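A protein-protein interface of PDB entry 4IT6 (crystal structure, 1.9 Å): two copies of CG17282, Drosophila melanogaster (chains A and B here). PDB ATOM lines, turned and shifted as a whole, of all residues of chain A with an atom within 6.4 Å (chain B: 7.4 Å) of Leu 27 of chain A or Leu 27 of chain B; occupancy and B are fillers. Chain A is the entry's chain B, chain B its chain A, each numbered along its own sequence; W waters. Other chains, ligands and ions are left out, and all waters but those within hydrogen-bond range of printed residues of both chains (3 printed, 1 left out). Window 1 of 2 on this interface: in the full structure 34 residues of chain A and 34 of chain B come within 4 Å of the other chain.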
ATOM      1  N   MET A   5      -6.630   9.439 -24.210  1.00  0.00           N
ATOM      2  CA  MET A   5      -5.399  10.209 -24.073  1.00  0.00           C
ATOM      3  C   MET A   5      -4.928  10.235 -22.622  1.00  0.00           C
ATOM      4  O   MET A   5      -5.695   9.945 -21.708  1.00  0.00           O
ATOM      5  CB  MET A   5      -5.598  11.637 -24.591  1.00  0.00           C
ATOM      6  CG  MET A   5      -5.831  11.730 -26.092  1.00  0.00           C
ATOM      7  SD  MET A   5      -6.173  13.547 -26.708  1.00  0.00           S
ATOM      8  CE  MET A   5      -6.467  13.167 -28.598  1.00  0.00           C
ATOM      9  N   ASP A   6      -3.662  10.584 -22.417  1.00  0.00           N
ATOM     10  CA  ASP A   6      -3.104  10.680 -21.073  1.00  0.00           C
ATOM     11  C   ASP A   6      -3.179  12.115 -20.556  1.00  0.00           C
ATOM     12  O   ASP A   6      -2.270  12.913 -20.771  1.00  0.00           O
ATOM     13  CB  ASP A   6      -1.657  10.184 -21.050  1.00  0.00           C
ATOM     14  CG  ASP A   6      -1.555   8.681 -21.218  1.00  0.00           C
ATOM     15  OD1 ASP A   6      -2.561   7.983 -20.975  1.00  0.00           O
ATOM     16  OD2 ASP A   6      -0.467   8.199 -21.595  1.00  0.00           O
ATOM     17  N   TRP A   7      -4.274  12.427 -19.872  1.00  0.00           N
ATOM     18  CA  TRP A   7      -4.517  13.771 -19.367  1.00  0.00           C
ATOM     19  C   TRP A   7      -3.849  14.017 -18.022  1.00  0.00           C
ATOM     20  O   TRP A   7      -3.672  13.097 -17.225  1.00  0.00           O
ATOM     21  CB  TRP A   7      -6.019  14.018 -19.228  1.00  0.00           C
ATOM     22  CG  TRP A   7      -6.790  13.813 -20.490  1.00  0.00           C
ATOM     23  CD1 TRP A   7      -7.248  12.631 -20.986  1.00  0.00           C
ATOM     24  CD2 TRP A   7      -7.204  14.825 -21.415  1.00  0.00           C
ATOM     25  NE1 TRP A   7      -7.919  12.841 -22.164  1.00  0.00           N
ATOM     26  CE2 TRP A   7      -7.907  14.180 -22.449  1.00  0.00           C
ATOM     27  CE3 TRP A   7      -7.046  16.211 -21.467  1.00  0.00           C
ATOM     28  CZ2 TRP A   7      -8.449  14.874 -23.526  1.00  0.00           C
ATOM     29  CZ3 TRP A   7      -7.586  16.899 -22.535  1.00  0.00           C
ATOM     30  CH2 TRP A   7      -8.280  16.230 -23.550  1.00  0.00           C
ATOM     31  N   TYR A   8      -3.494  15.272 -17.771  1.00  0.00           N
ATOM     32  CA  TYR A   8      -2.965  15.672 -16.476  1.00  0.00           C
ATOM     33  C   TYR A   8      -3.953  16.595 -15.773  1.00  0.00           C
ATOM     34  O   TYR A   8      -4.269  16.400 -14.603  1.00  0.00           O
ATOM     35  CB  TYR A   8      -1.608  16.363 -16.620  1.00  0.00           C
ATOM     36  CG  TYR A   8      -0.951  16.650 -15.290  1.00  0.00           C
ATOM     37  CD1 TYR A   8      -0.580  15.615 -14.443  1.00  0.00           C
ATOM     38  CD2 TYR A   8      -0.716  17.951 -14.874  1.00  0.00           C
ATOM     39  CE1 TYR A   8       0.014  15.867 -13.224  1.00  0.00           C
ATOM     40  CE2 TYR A   8      -0.121  18.213 -13.655  1.00  0.00           C
ATOM     41  CZ  TYR A   8       0.241  17.166 -12.834  1.00  0.00           C
ATOM     42  OH  TYR A   8       0.832  17.417 -11.619  1.00  0.00           O
ATOM     43  N   VAL A   9      -4.432  17.601 -16.493  1.00  0.00           N
ATOM     44  CA  VAL A   9      -5.437  18.501 -15.955  1.00  0.00           C
ATOM     45  C   VAL A   9      -6.651  17.674 -15.556  1.00  0.00           C
ATOM     46  O   VAL A   9      -7.058  16.768 -16.280  1.00  0.00           O
ATOM     47  CB  VAL A   9      -5.843  19.575 -16.978  1.00  0.00           C
ATOM     48  CG1 VAL A   9      -7.062  20.338 -16.492  1.00  0.00           C
ATOM     49  CG2 VAL A   9      -4.682  20.521 -17.237  1.00  0.00           C
ATOM     50  N   VAL A  24      -5.521  19.381 -10.203  1.00  0.00           N
ATOM     51  CA  VAL A  24      -4.962  20.167 -11.296  1.00  0.00           C
ATOM     52  C   VAL A  24      -6.091  20.802 -12.094  1.00  0.00           C
ATOM     53  O   VAL A  24      -6.994  20.107 -12.549  1.00  0.00           O
ATOM     54  CB  VAL A  24      -4.106  19.302 -12.234  1.00  0.00           C
ATOM     55  CG1 VAL A  24      -3.407  20.172 -13.268  1.00  0.00           C
ATOM     56  CG2 VAL A  24      -3.100  18.486 -11.437  1.00  0.00           C
ATOM     57  N   ILE A  25      -6.046  22.119 -12.263  1.00  0.00           N
ATOM     58  CA  ILE A  25      -7.136  22.797 -12.941  1.00  0.00           C
ATOM     59  C   ILE A  25      -6.623  23.525 -14.154  1.00  0.00           C
ATOM     60  O   ILE A  25      -7.410  24.014 -14.965  1.00  0.00           O
ATOM     61  CB  ILE A  25      -7.887  23.813 -12.039  1.00  0.00           C
ATOM     62  CG1 ILE A  25      -6.930  24.862 -11.479  1.00  0.00           C
ATOM     63  CG2 ILE A  25      -8.607  23.107 -10.926  1.00  0.00           C
ATOM     64  CD1 ILE A  25      -7.673  25.996 -10.788  1.00  0.00           C
ATOM     65  N   GLY A  26      -5.301  23.614 -14.274  1.00  0.00           N
ATOM     66  CA  GLY A  26      -4.724  24.232 -15.451  1.00  0.00           C
ATOM     67  C   GLY A  26      -3.243  23.971 -15.627  1.00  0.00           C
ATOM     68  O   GLY A  26      -2.538  23.663 -14.654  1.00  0.00           O
ATOM     69  N   LEU A  27      -2.789  24.110 -16.869  1.00  0.00           N
ATOM     70  CA  LEU A  27      -1.384  23.997 -17.224  1.00  0.00           C
ATOM     71  C   LEU A  27      -1.008  25.142 -18.158  1.00  0.00           C
ATOM     72  O   LEU A  27      -1.688  25.390 -19.151  1.00  0.00           O
ATOM     73  CB  LEU A  27      -1.111  22.664 -17.917  1.00  0.00           C
ATOM     74  CG  LEU A  27      -0.900  21.436 -17.033  1.00  0.00           C
ATOM     75  CD1 LEU A  27      -0.776  20.194 -17.898  1.00  0.00           C
ATOM     76  CD2 LEU A  27       0.333  21.606 -16.162  1.00  0.00           C
ATOM     77  N   GLN A  28       0.075  25.835 -17.830  1.00  0.00           N
ATOM     78  CA  GLN A  28       0.566  26.927 -18.658  1.00  0.00           C
ATOM     79  C   GLN A  28       2.077  26.828 -18.798  1.00  0.00           C
ATOM     80  O   GLN A  28       2.820  27.189 -17.888  1.00  0.00           O
ATOM     81  CB  GLN A  28       0.180  28.279 -18.061  1.00  0.00           C
ATOM     82  CG  GLN A  28      -1.264  28.671 -18.306  1.00  0.00           C
ATOM     83  CD  GLN A  28      -1.741  29.760 -17.365  1.00  0.00           C
ATOM     84  OE1 GLN A  28      -1.387  29.779 -16.187  1.00  0.00           O
ATOM     85  NE2 GLN A  28      -2.548  30.675 -17.884  1.00  0.00           N
ATOM     86  N   PHE A  29       2.524  26.326 -19.942  1.00  0.00           N
ATOM     87  CA  PHE A  29       3.947  26.148 -20.191  1.00  0.00           C
ATOM     88  C   PHE A  29       4.514  27.322 -20.974  1.00  0.00           C
ATOM     89  O   PHE A  29       3.796  27.991 -21.714  1.00  0.00           O
ATOM     90  CB  PHE A  29       4.196  24.838 -20.937  1.00  0.00           C
ATOM     91  CG  PHE A  29       3.740  23.621 -20.186  1.00  0.00           C
ATOM     92  CD1 PHE A  29       4.261  23.328 -18.939  1.00  0.00           C
ATOM     93  CD2 PHE A  29       2.790  22.774 -20.721  1.00  0.00           C
ATOM     94  CE1 PHE A  29       3.848  22.214 -18.247  1.00  0.00           C
ATOM     95  CE2 PHE A  29       2.372  21.657 -20.030  1.00  0.00           C
ATOM     96  CZ  PHE A  29       2.902  21.378 -18.793  1.00  0.00           C
ATOM     97  N   VAL A  95       7.314  19.703 -23.961  1.00  0.00           N
ATOM     98  CA  VAL A  95       7.807  19.709 -22.581  1.00  0.00           C
ATOM     99  C   VAL A  95       8.113  18.259 -22.180  1.00  0.00           C
ATOM    100  O   VAL A  95       7.481  17.334 -22.698  1.00  0.00           O
ATOM    101  CB  VAL A  95       6.789  20.339 -21.593  1.00  0.00           C
ATOM    102  CG1 VAL A  95       6.372  21.698 -22.098  1.00  0.00           C
ATOM    103  CG2 VAL A  95       5.559  19.455 -21.479  1.00  0.00           C
ATOM    104  N   PRO A  96       9.110  18.050 -21.300  1.00  0.00           N
ATOM    105  CA  PRO A  96       9.470  16.688 -20.867  1.00  0.00           C
ATOM    106  C   PRO A  96       8.248  16.012 -20.286  1.00  0.00           C
ATOM    107  O   PRO A  96       7.599  16.613 -19.430  1.00  0.00           O
ATOM    108  CB  PRO A  96      10.463  16.928 -19.738  1.00  0.00           C
ATOM    109  CG  PRO A  96      11.104  18.242 -20.088  1.00  0.00           C
ATOM    110  CD  PRO A  96      10.005  19.076 -20.733  1.00  0.00           C
ATOM    111  N   GLY A  97       7.930  14.803 -20.756  1.00  0.00           N
ATOM    112  CA  GLY A  97       6.737  14.094 -20.323  1.00  0.00           C
ATOM    113  C   GLY A  97       5.594  14.117 -21.329  1.00  0.00           C
ATOM    114  O   GLY A  97       4.609  13.425 -21.162  1.00  0.00           O
ATOM    115  N   GLU A  98       5.729  14.930 -22.368  1.00  0.00           N
ATOM    116  CA  GLU A  98       4.723  15.067 -23.421  1.00  0.00           C
ATOM    117  C   GLU A  98       4.866  14.062 -24.577  1.00  0.00           C
ATOM    118  O   GLU A  98       5.968  13.820 -25.099  1.00  0.00           O
ATOM    119  CB  GLU A  98       4.799  16.485 -24.004  1.00  0.00           C
ATOM    120  CG  GLU A  98       4.026  16.668 -25.307  1.00  0.00           C
ATOM    121  CD  GLU A  98       4.147  18.087 -25.846  1.00  0.00           C
ATOM    122  OE1 GLU A  98       4.810  18.935 -25.186  1.00  0.00           O
ATOM    123  OE2 GLU A  98       3.596  18.363 -26.937  1.00  0.00           O
ATOM    124  N   THR A  99       3.743  13.475 -24.977  1.00  0.00           N
ATOM    125  CA  THR A  99       3.672  12.656 -26.178  1.00  0.00           C
ATOM    126  C   THR A  99       2.805  13.435 -27.150  1.00  0.00           C
ATOM    127  O   THR A  99       1.781  13.980 -26.770  1.00  0.00           O
ATOM    128  CB  THR A  99       3.059  11.262 -25.880  1.00  0.00           C
ATOM    129  OG1 THR A  99       3.860  10.587 -24.900  1.00  0.00           O
ATOM    130  CG2 THR A  99       3.016  10.389 -27.145  1.00  0.00           C
ATOM    131  N   ASP B   6      -5.095  26.673 -19.365  1.00  0.00           N
ATOM    132  CA  ASP B   6      -5.987  25.584 -18.986  1.00  0.00           C
ATOM    133  C   ASP B   6      -5.488  24.230 -19.493  1.00  0.00           C
ATOM    134  O   ASP B   6      -4.501  23.699 -18.989  1.00  0.00           O
ATOM    135  CB  ASP B   6      -7.409  25.852 -19.486  1.00  0.00           C
ATOM    136  CG  ASP B   6      -8.402  26.037 -18.354  1.00  0.00           C
ATOM    137  OD1 ASP B   6      -8.347  25.263 -17.375  1.00  0.00           O
ATOM    138  OD2 ASP B   6      -9.240  26.959 -18.444  1.00  0.00           O
ATOM    139  N   TRP B   7      -6.175  23.680 -20.489  1.00  0.00           N
ATOM    140  CA  TRP B   7      -5.858  22.355 -21.015  1.00  0.00           C
ATOM    141  C   TRP B   7      -4.655  22.371 -21.952  1.00  0.00           C
ATOM    142  O   TRP B   7      -4.520  23.262 -22.787  1.00  0.00           O
ATOM    143  CB  TRP B   7      -7.066  21.762 -21.744  1.00  0.00           C
ATOM    144  CG  TRP B   7      -8.286  21.644 -20.892  1.00  0.00           C
ATOM    145  CD1 TRP B   7      -9.315  22.533 -20.808  1.00  0.00           C
ATOM    146  CD2 TRP B   7      -8.609  20.571 -19.999  1.00  0.00           C
ATOM    147  NE1 TRP B   7     -10.259  22.083 -19.919  1.00  0.00           N
ATOM    148  CE2 TRP B   7      -9.850  20.880 -19.408  1.00  0.00           C
ATOM    149  CE3 TRP B   7      -7.971  19.381 -19.643  1.00  0.00           C
ATOM    150  CZ2 TRP B   7     -10.462  20.045 -18.480  1.00  0.00           C
ATOM    151  CZ3 TRP B   7      -8.582  18.551 -18.723  1.00  0.00           C
ATOM    152  CH2 TRP B   7      -9.815  18.887 -18.152  1.00  0.00           C
ATOM    153  N   TYR B   8      -3.789  21.373 -21.815  1.00  0.00           N
ATOM    154  CA  TYR B   8      -2.637  21.240 -22.694  1.00  0.00           C
ATOM    155  C   TYR B   8      -2.830  20.078 -23.649  1.00  0.00           C
ATOM    156  O   TYR B   8      -2.685  20.224 -24.859  1.00  0.00           O
ATOM    157  CB  TYR B   8      -1.351  21.042 -21.897  1.00  0.00           C
ATOM    158  CG  TYR B   8      -0.118  21.064 -22.766  1.00  0.00           C
ATOM    159  CD1 TYR B   8       0.243  22.213 -23.458  1.00  0.00           C
ATOM    160  CD2 TYR B   8       0.676  19.938 -22.910  1.00  0.00           C
ATOM    161  CE1 TYR B   8       1.364  22.241 -24.260  1.00  0.00           C
ATOM    162  CE2 TYR B   8       1.799  19.958 -23.710  1.00  0.00           C
ATOM    163  CZ  TYR B   8       2.139  21.112 -24.382  1.00  0.00           C
ATOM    164  OH  TYR B   8       3.258  21.138 -25.180  1.00  0.00           O
ATOM    165  N   VAL B   9      -3.154  18.916 -23.098  1.00  0.00           N
ATOM    166  CA  VAL B   9      -3.429  17.760 -23.929  1.00  0.00           C
ATOM    167  C   VAL B   9      -4.548  18.134 -24.884  1.00  0.00           C
ATOM    168  O   VAL B   9      -5.538  18.748 -24.490  1.00  0.00           O
ATOM    169  CB  VAL B   9      -3.824  16.535 -23.096  1.00  0.00           C
ATOM    170  CG1 VAL B   9      -4.502  15.498 -23.972  1.00  0.00           C
ATOM    171  CG2 VAL B   9      -2.599  15.949 -22.416  1.00  0.00           C
ATOM    172  N   VAL B  24      -0.752  17.443 -29.031  1.00  0.00           N
ATOM    173  CA  VAL B  24      -0.407  16.787 -27.756  1.00  0.00           C
ATOM    174  C   VAL B  24      -1.450  15.707 -27.492  1.00  0.00           C
ATOM    175  O   VAL B  24      -2.649  15.969 -27.548  1.00  0.00           O
ATOM    176  CB  VAL B  24      -0.416  17.810 -26.596  1.00  0.00           C
ATOM    177  CG1 VAL B  24      -0.030  17.141 -25.234  1.00  0.00           C
ATOM    178  CG2 VAL B  24       0.502  18.996 -26.914  1.00  0.00           C
ATOM    179  N   ILE B  25      -1.010  14.494 -27.210  1.00  0.00           N
ATOM    180  CA  ILE B  25      -1.965  13.423 -26.978  1.00  0.00           C
ATOM    181  C   ILE B  25      -1.783  12.832 -25.591  1.00  0.00           C
ATOM    182  O   ILE B  25      -2.585  12.020 -25.139  1.00  0.00           O
ATOM    183  CB  ILE B  25      -1.849  12.291 -28.035  1.00  0.00           C
ATOM    184  CG1 ILE B  25      -0.443  11.692 -28.032  1.00  0.00           C
ATOM    185  CG2 ILE B  25      -2.147  12.829 -29.413  1.00  0.00           C
ATOM    186  CD1 ILE B  25      -0.338  10.466 -28.957  1.00  0.00           C
ATOM    187  N   GLY B  26      -0.712  13.225 -24.911  1.00  0.00           N
ATOM    188  CA  GLY B  26      -0.439  12.673 -23.598  1.00  0.00           C
ATOM    189  C   GLY B  26       0.555  13.445 -22.758  1.00  0.00           C
ATOM    190  O   GLY B  26       1.458  14.099 -23.277  1.00  0.00           O
ATOM    191  N   LEU B  27       0.376  13.356 -21.445  1.00  0.00           N
ATOM    192  CA  LEU B  27       1.279  13.974 -20.487  1.00  0.00           C
ATOM    193  C   LEU B  27       1.535  13.018 -19.330  1.00  0.00           C
ATOM    194  O   LEU B  27       0.608  12.635 -18.619  1.00  0.00           O
ATOM    195  CB  LEU B  27       0.688  15.279 -19.954  1.00  0.00           C
ATOM    196  CG  LEU B  27       1.004  16.559 -20.726  1.00  0.00           C
ATOM    197  CD1 LEU B  27       0.430  17.768 -20.006  1.00  0.00           C
ATOM    198  CD2 LEU B  27       2.501  16.711 -20.925  1.00  0.00           C
ATOM    199  N   GLN B  28       2.793  12.638 -19.146  1.00  0.00           N
ATOM    200  CA  GLN B  28       3.179  11.767 -18.045  1.00  0.00           C
ATOM    201  C   GLN B  28       4.353  12.370 -17.282  1.00  0.00           C
ATOM    202  O   GLN B  28       5.487  12.349 -17.755  1.00  0.00           O
ATOM    203  CB  GLN B  28       3.547  10.373 -18.557  1.00  0.00           C
ATOM    204  CG  GLN B  28       2.352   9.503 -18.916  1.00  0.00           C
ATOM    205  CD  GLN B  28       1.538   9.096 -17.701  1.00  0.00           C
ATOM    206  OE1 GLN B  28       0.349   9.398 -17.607  1.00  0.00           O
ATOM    207  NE2 GLN B  28       2.178   8.408 -16.765  1.00  0.00           N
ATOM    208  N   PHE B  29       4.073  12.912 -16.102  1.00  0.00           N
ATOM    209  CA  PHE B  29       5.103  13.535 -15.292  1.00  0.00           C
ATOM    210  C   PHE B  29       5.609  12.558 -14.242  1.00  0.00           C
ATOM    211  O   PHE B  29       4.911  11.619 -13.865  1.00  0.00           O
ATOM    212  CB  PHE B  29       4.574  14.818 -14.650  1.00  0.00           C
ATOM    213  CG  PHE B  29       4.173  15.872 -15.645  1.00  0.00           C
ATOM    214  CD1 PHE B  29       5.095  16.362 -16.548  1.00  0.00           C
ATOM    215  CD2 PHE B  29       2.875  16.359 -15.687  1.00  0.00           C
ATOM    216  CE1 PHE B  29       4.749  17.324 -17.461  1.00  0.00           C
ATOM    217  CE2 PHE B  29       2.518  17.319 -16.599  1.00  0.00           C
ATOM    218  CZ  PHE B  29       3.450  17.804 -17.497  1.00  0.00           C
ATOM    219  N   VAL B  95       4.037  20.399 -10.991  1.00  0.00           N
ATOM    220  CA  VAL B  95       5.051  20.684 -12.006  1.00  0.00           C
ATOM    221  C   VAL B  95       4.999  22.181 -12.356  1.00  0.00           C
ATOM    222  O   VAL B  95       3.931  22.806 -12.269  1.00  0.00           O
ATOM    223  CB  VAL B  95       4.882  19.813 -13.281  1.00  0.00           C
ATOM    224  CG1 VAL B  95       4.796  18.343 -12.905  1.00  0.00           C
ATOM    225  CG2 VAL B  95       3.628  20.219 -14.032  1.00  0.00           C
ATOM    226  N   PRO B  96       6.154  22.769 -12.719  1.00  0.00           N
ATOM    227  CA  PRO B  96       6.194  24.195 -13.074  1.00  0.00           C
ATOM    228  C   PRO B  96       5.216  24.443 -14.190  1.00  0.00           C
ATOM    229  O   PRO B  96       5.291  23.766 -15.219  1.00  0.00           O
ATOM    230  CB  PRO B  96       7.612  24.394 -13.609  1.00  0.00           C
ATOM    231  CG  PRO B  96       8.423  23.334 -12.880  1.00  0.00           C
ATOM    232  CD  PRO B  96       7.494  22.150 -12.709  1.00  0.00           C
ATOM    233  N   GLY B  97       4.316  25.404 -13.987  1.00  0.00           N
ATOM    234  CA  GLY B  97       3.289  25.725 -14.958  1.00  0.00           C
ATOM    235  C   GLY B  97       1.895  25.267 -14.556  1.00  0.00           C
ATOM    236  O   GLY B  97       0.922  25.633 -15.181  1.00  0.00           O
ATOM    237  N   GLU B  98       1.819  24.466 -13.499  1.00  0.00           N
ATOM    238  CA  GLU B  98       0.553  23.897 -13.054  1.00  0.00           C
ATOM    239  C   GLU B  98      -0.165  24.747 -12.006  1.00  0.00           C
ATOM    240  O   GLU B  98       0.438  25.204 -11.038  1.00  0.00           O
ATOM    241  CB  GLU B  98       0.771  22.481 -12.512  1.00  0.00           C
ATOM    242  CG  GLU B  98      -0.284  22.026 -11.517  1.00  0.00           C
ATOM    243  CD  GLU B  98       0.076  20.717 -10.833  1.00  0.00           C
ATOM    244  OE1 GLU B  98       1.179  20.191 -11.085  1.00  0.00           O
ATOM    245  OE2 GLU B  98      -0.746  20.214 -10.041  1.00  0.00           O
ATOM    246  N   THR B  99      -1.463  24.942 -12.218  1.00  0.00           N
ATOM    247  CA  THR B  99      -2.345  25.566 -11.250  1.00  0.00           C
ATOM    248  C   THR B  99      -3.250  24.462 -10.719  1.00  0.00           C
ATOM    249  O   THR B  99      -3.787  23.655 -11.504  1.00  0.00           O
ATOM    250  CB  THR B  99      -3.195  26.676 -11.914  1.00  0.00           C
ATOM    251  OG1 THR B  99      -2.317  27.644 -12.507  1.00  0.00           O
ATOM    252  CG2 THR B  99      -4.088  27.374 -10.874  1.00  0.00           C
ATOM    253  N   LYS B 117      -0.313  28.349  -8.125  1.00  0.00           N
ATOM    254  CA  LYS B 117       0.390  28.022  -9.366  1.00  0.00           C
ATOM    255  C   LYS B 117       1.892  27.902  -9.104  1.00  0.00           C
ATOM    256  O   LYS B 117       2.467  28.789  -8.494  1.00  0.00           O
ATOM    257  CB  LYS B 117       0.168  29.083 -10.432  1.00  0.00           C
ATOM    258  CG  LYS B 117       0.986  28.808 -11.714  1.00  0.00           C
ATOM    259  CD  LYS B 117       0.675  29.834 -12.799  1.00  0.00           C
ATOM    260  CE  LYS B 117       1.512  29.572 -14.078  1.00  0.00           C
ATOM    261  NZ  LYS B 117       1.313  30.670 -15.064  1.00  0.00           N
HETATM  262  O   HOH W   1      -1.368  27.336 -14.957  1.00  0.00           O
HETATM  263  O   HOH W   2       8.233  13.624 -17.756  1.00  0.00           O
HETATM  264  O   HOH W   3       5.571  26.783 -16.661  1.00  0.00           O
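Water W1 lies within hydrogen-bond range of OG1 of Thr 99 of chain B (2.6 Å), OE1 of Gln 28 of chain A (2.7 Å) and O of Gly 97 of chain B (2.9 Å).
Water W2 lies within hydrogen-bond range of O of Gln 28 of chain B (3.0 Å), N of Gly 97 of chain A (3.2 Å) and O of Pro 96 of chain A (3.5 Å).
Water W3 lies within hydrogen-bond range of the backbone carbonyl oxygen of Gln 28 of chain A (3.0 Å), the backbone NH of Gly 97 of chain B (3.3 Å) and the backbone carbonyl oxygen of Pro 96 of chain B (3.4 Å).
Leu 27 of chain A touches just these residues of chain B: Asp 6 (2.8 Å), Leu 27 (3.4 Å), Gly 97 (3.5 Å) and Glu 98 (3.8 Å).
Of chain A, only Asp 6, Leu 27, Gly 97 and Glu 98 come within 4 Å of Leu 27 of chain B.
Of the printed residues of chain B, Val 9 of chain A touches Asp 6 and Trp 7.
Printed residues of chain B within 4 Å of Trp 7 of chain A: Trp 7 and Val 9.
Of the printed residues of chain B, Gln 28 of chain A touches Gly 97 (2.8 Å) and Lys 117 (3.1 Å).
Of the printed residues of chain B, Gly 97 of chain A touches Gly 26, Leu 27 and Gln 28.
The nearest printed residue of chain A that does not touch Val 9 of chain B is Tyr 8 of chain A (4.8 Å).
Asp 6 of chain A touches Ile 25 of chain B, and with the chains exchanged Ile 25 of chain A touches Asp 6 of chain B.
Asp 6 of chain A touches Leu 27 of chain B, and with the chains exchanged Leu 27 of chain A touches Asp 6 of chain B.
Trp 7 of chain A touches Val 9 of chain B, and with the chains exchanged Val 9 of chain A touches Trp 7 of chain B.
Val 24 of chain A touches Glu 98 of chain B, and with the chains exchanged Glu 98 of chain A touches Val 24 of chain B.
15 positions are printed for both chains.
Of the 39 pairs that touch across the chains among the printed residues, 35 have their exchanged pair printed and touching as well.
OE1 of Glu 98 of chain B is in hydrogen-bond range of N of Val 95 of chain B (2.9 Å).
The side-chain carboxylate (OE1) of Glu 98 of chain A is in hydrogen-bond range of the backbone NH (N) of Val 95 of chain A.
Among the printed residues, merely in contact across the chains: Met 5 of chain A with Val 9 of chain B (3.8 Å), Met 5 of chain A with Ile 25 of chain B (3.1 Å), Asp 6 of chain A with Val 9 of chain B (3.5 Å), Asp 6 of chain A with Gly 26 of chain B (3.4 Å), Trp 7 of chain A with Trp 7 of chain B (3.8 Å), Trp 7 of chain A with Val 9 of chain B (3.4 Å), Tyr 8 of chain A with Phe 29 of chain B (3.7 Å), Val 9 of chain A with Asp 6 of chain B (3.6 Å), Val 9 of chain A with Trp 7 of chain B (3.2 Å), Val 24 of chain A with Glu 98 of chain B (3.2 Å), Val 24 of chain A with Thr 99 of chain B (3.7 Å), Gly 26 of chain A with Asp 6 of chain B (3.6 Å), Gly 26 of chain A with Glu 98 of chain B (3.5 Å), Leu 27 of chain A with Leu 27 of chain B (3.4 Å), Leu 27 of chain A with Gly 97 of chain B (3.5 Å), Leu 27 of chain A with Glu 98 of chain B (3.8 Å), Phe 29 of chain A with Tyr 8 of chain B (3.7 Å), Phe 29 of chain A with Phe 29 of chain B (3.8 Å), Phe 29 of chain A with Pro 96 of chain B (3.7 Å), Pro 96 of chain A with Phe 29 of chain B (3.5 Å), Gly 97 of chain A with Gly 26 of chain B (3.9 Å), Gly 97 of chain A with Leu 27 of chain B (3.4 Å), Glu 98 of chain A with Val 24 of chain B (3.2 Å), Glu 98 of chain A with Gly 26 of chain B (3.4 Å), Glu 98 of chain A with Leu 27 of chain B (3.7 Å) and Thr 99 of chain A with Val 24 of chain B (3.7 Å).
Printed residues of chain B that touch a printed residue of chain A: Asp 6, Trp 7, Tyr 8, Val 9, Val 24, Ile 25, Gly 26, Leu 27, Gln 28, Phe 29, Pro 96, Gly 97, Glu 98, Thr 99 and Lys 117.
Hydrophobic or aromatic side chains of chain B that line the printed part of chain A: Trp 7, Tyr 8, Val 9, Val 24, Ile 25, Leu 27 and Phe 29.
Hydrophobic or aromatic side chains of chain A within 4 Å of the printed part of chain B: Met 5, Trp 7, Tyr 8, Val 9, Val 24, Ile 25, Leu 27 and Phe 29.
Along chain A the printed residues that touch a printed residue of chain B span positions 5 to 99.
Among the printed residues, 39 pairs touch across the chains.
Among the printed residues, no Asp or Glu carboxylate lies within 4 Å of a Lys or Arg side-chain nitrogen of the other chain.
The backbone carbonyl oxygen of Asp 6 of chain B is in hydrogen-bond range of the backbone NH of Leu 27 of chain A.
The side-chain carboxylate (OE1) of Glu 98 of chain A is in hydrogen-bond range of the side-chain hydroxyl (OH) of Tyr 8 of chain B (2.7 Å).
O of Ile 25 of chain B sits at hydrogen-bond distance from N of Asp 6 of chain A (3.3 Å).
The backbone NH (N) of Ile 25 of chain B lies within hydrogen-bond range of the backbone carbonyl oxygen (O) of Thr 99 of chain A, at 2.9 Å.
O of Gly 26 of chain B lies within hydrogen-bond range of N of Thr 99 of chain A (2.9 Å).
O of Asp 6 of chain A is in hydrogen-bond range of N of Leu 27 of chain B (2.8 Å).
The backbone NH (N) of Gln 28 of chain B is in hydrogen-bond range of the backbone carbonyl oxygen (O) of Gly 97 of chain A.
The backbone NH of Gln 28 of chain A sits at hydrogen-bond distance from the backbone carbonyl oxygen of Gly 97 of chain B, 2.8 Å away.
OH of Tyr 8 of chain A sits at hydrogen-bond distance from OE1 of Glu 98 of chain B (2.8 Å).
The backbone carbonyl oxygen (O) of Thr 99 of chain B lies within hydrogen-bond range of the backbone NH (N) of Ile 25 of chain A.
The backbone NH (N) of Thr 99 of chain B sits at hydrogen-bond distance from the backbone carbonyl oxygen (O) of Gly 26 of chain A (3.0 Å).
The side-chain amino group (NZ) of Lys 117 of chain B sits at hydrogen-bond distance from the side-chain amide oxygen (OE1) of Gln 28 of chain A, at 3.1 Å.
The side-chain carboxylate (OD1) of Asp 6 of chain B sits close to the backbone carbonyl oxygen (O) of Ile 25 of chain A (2.9 Å).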
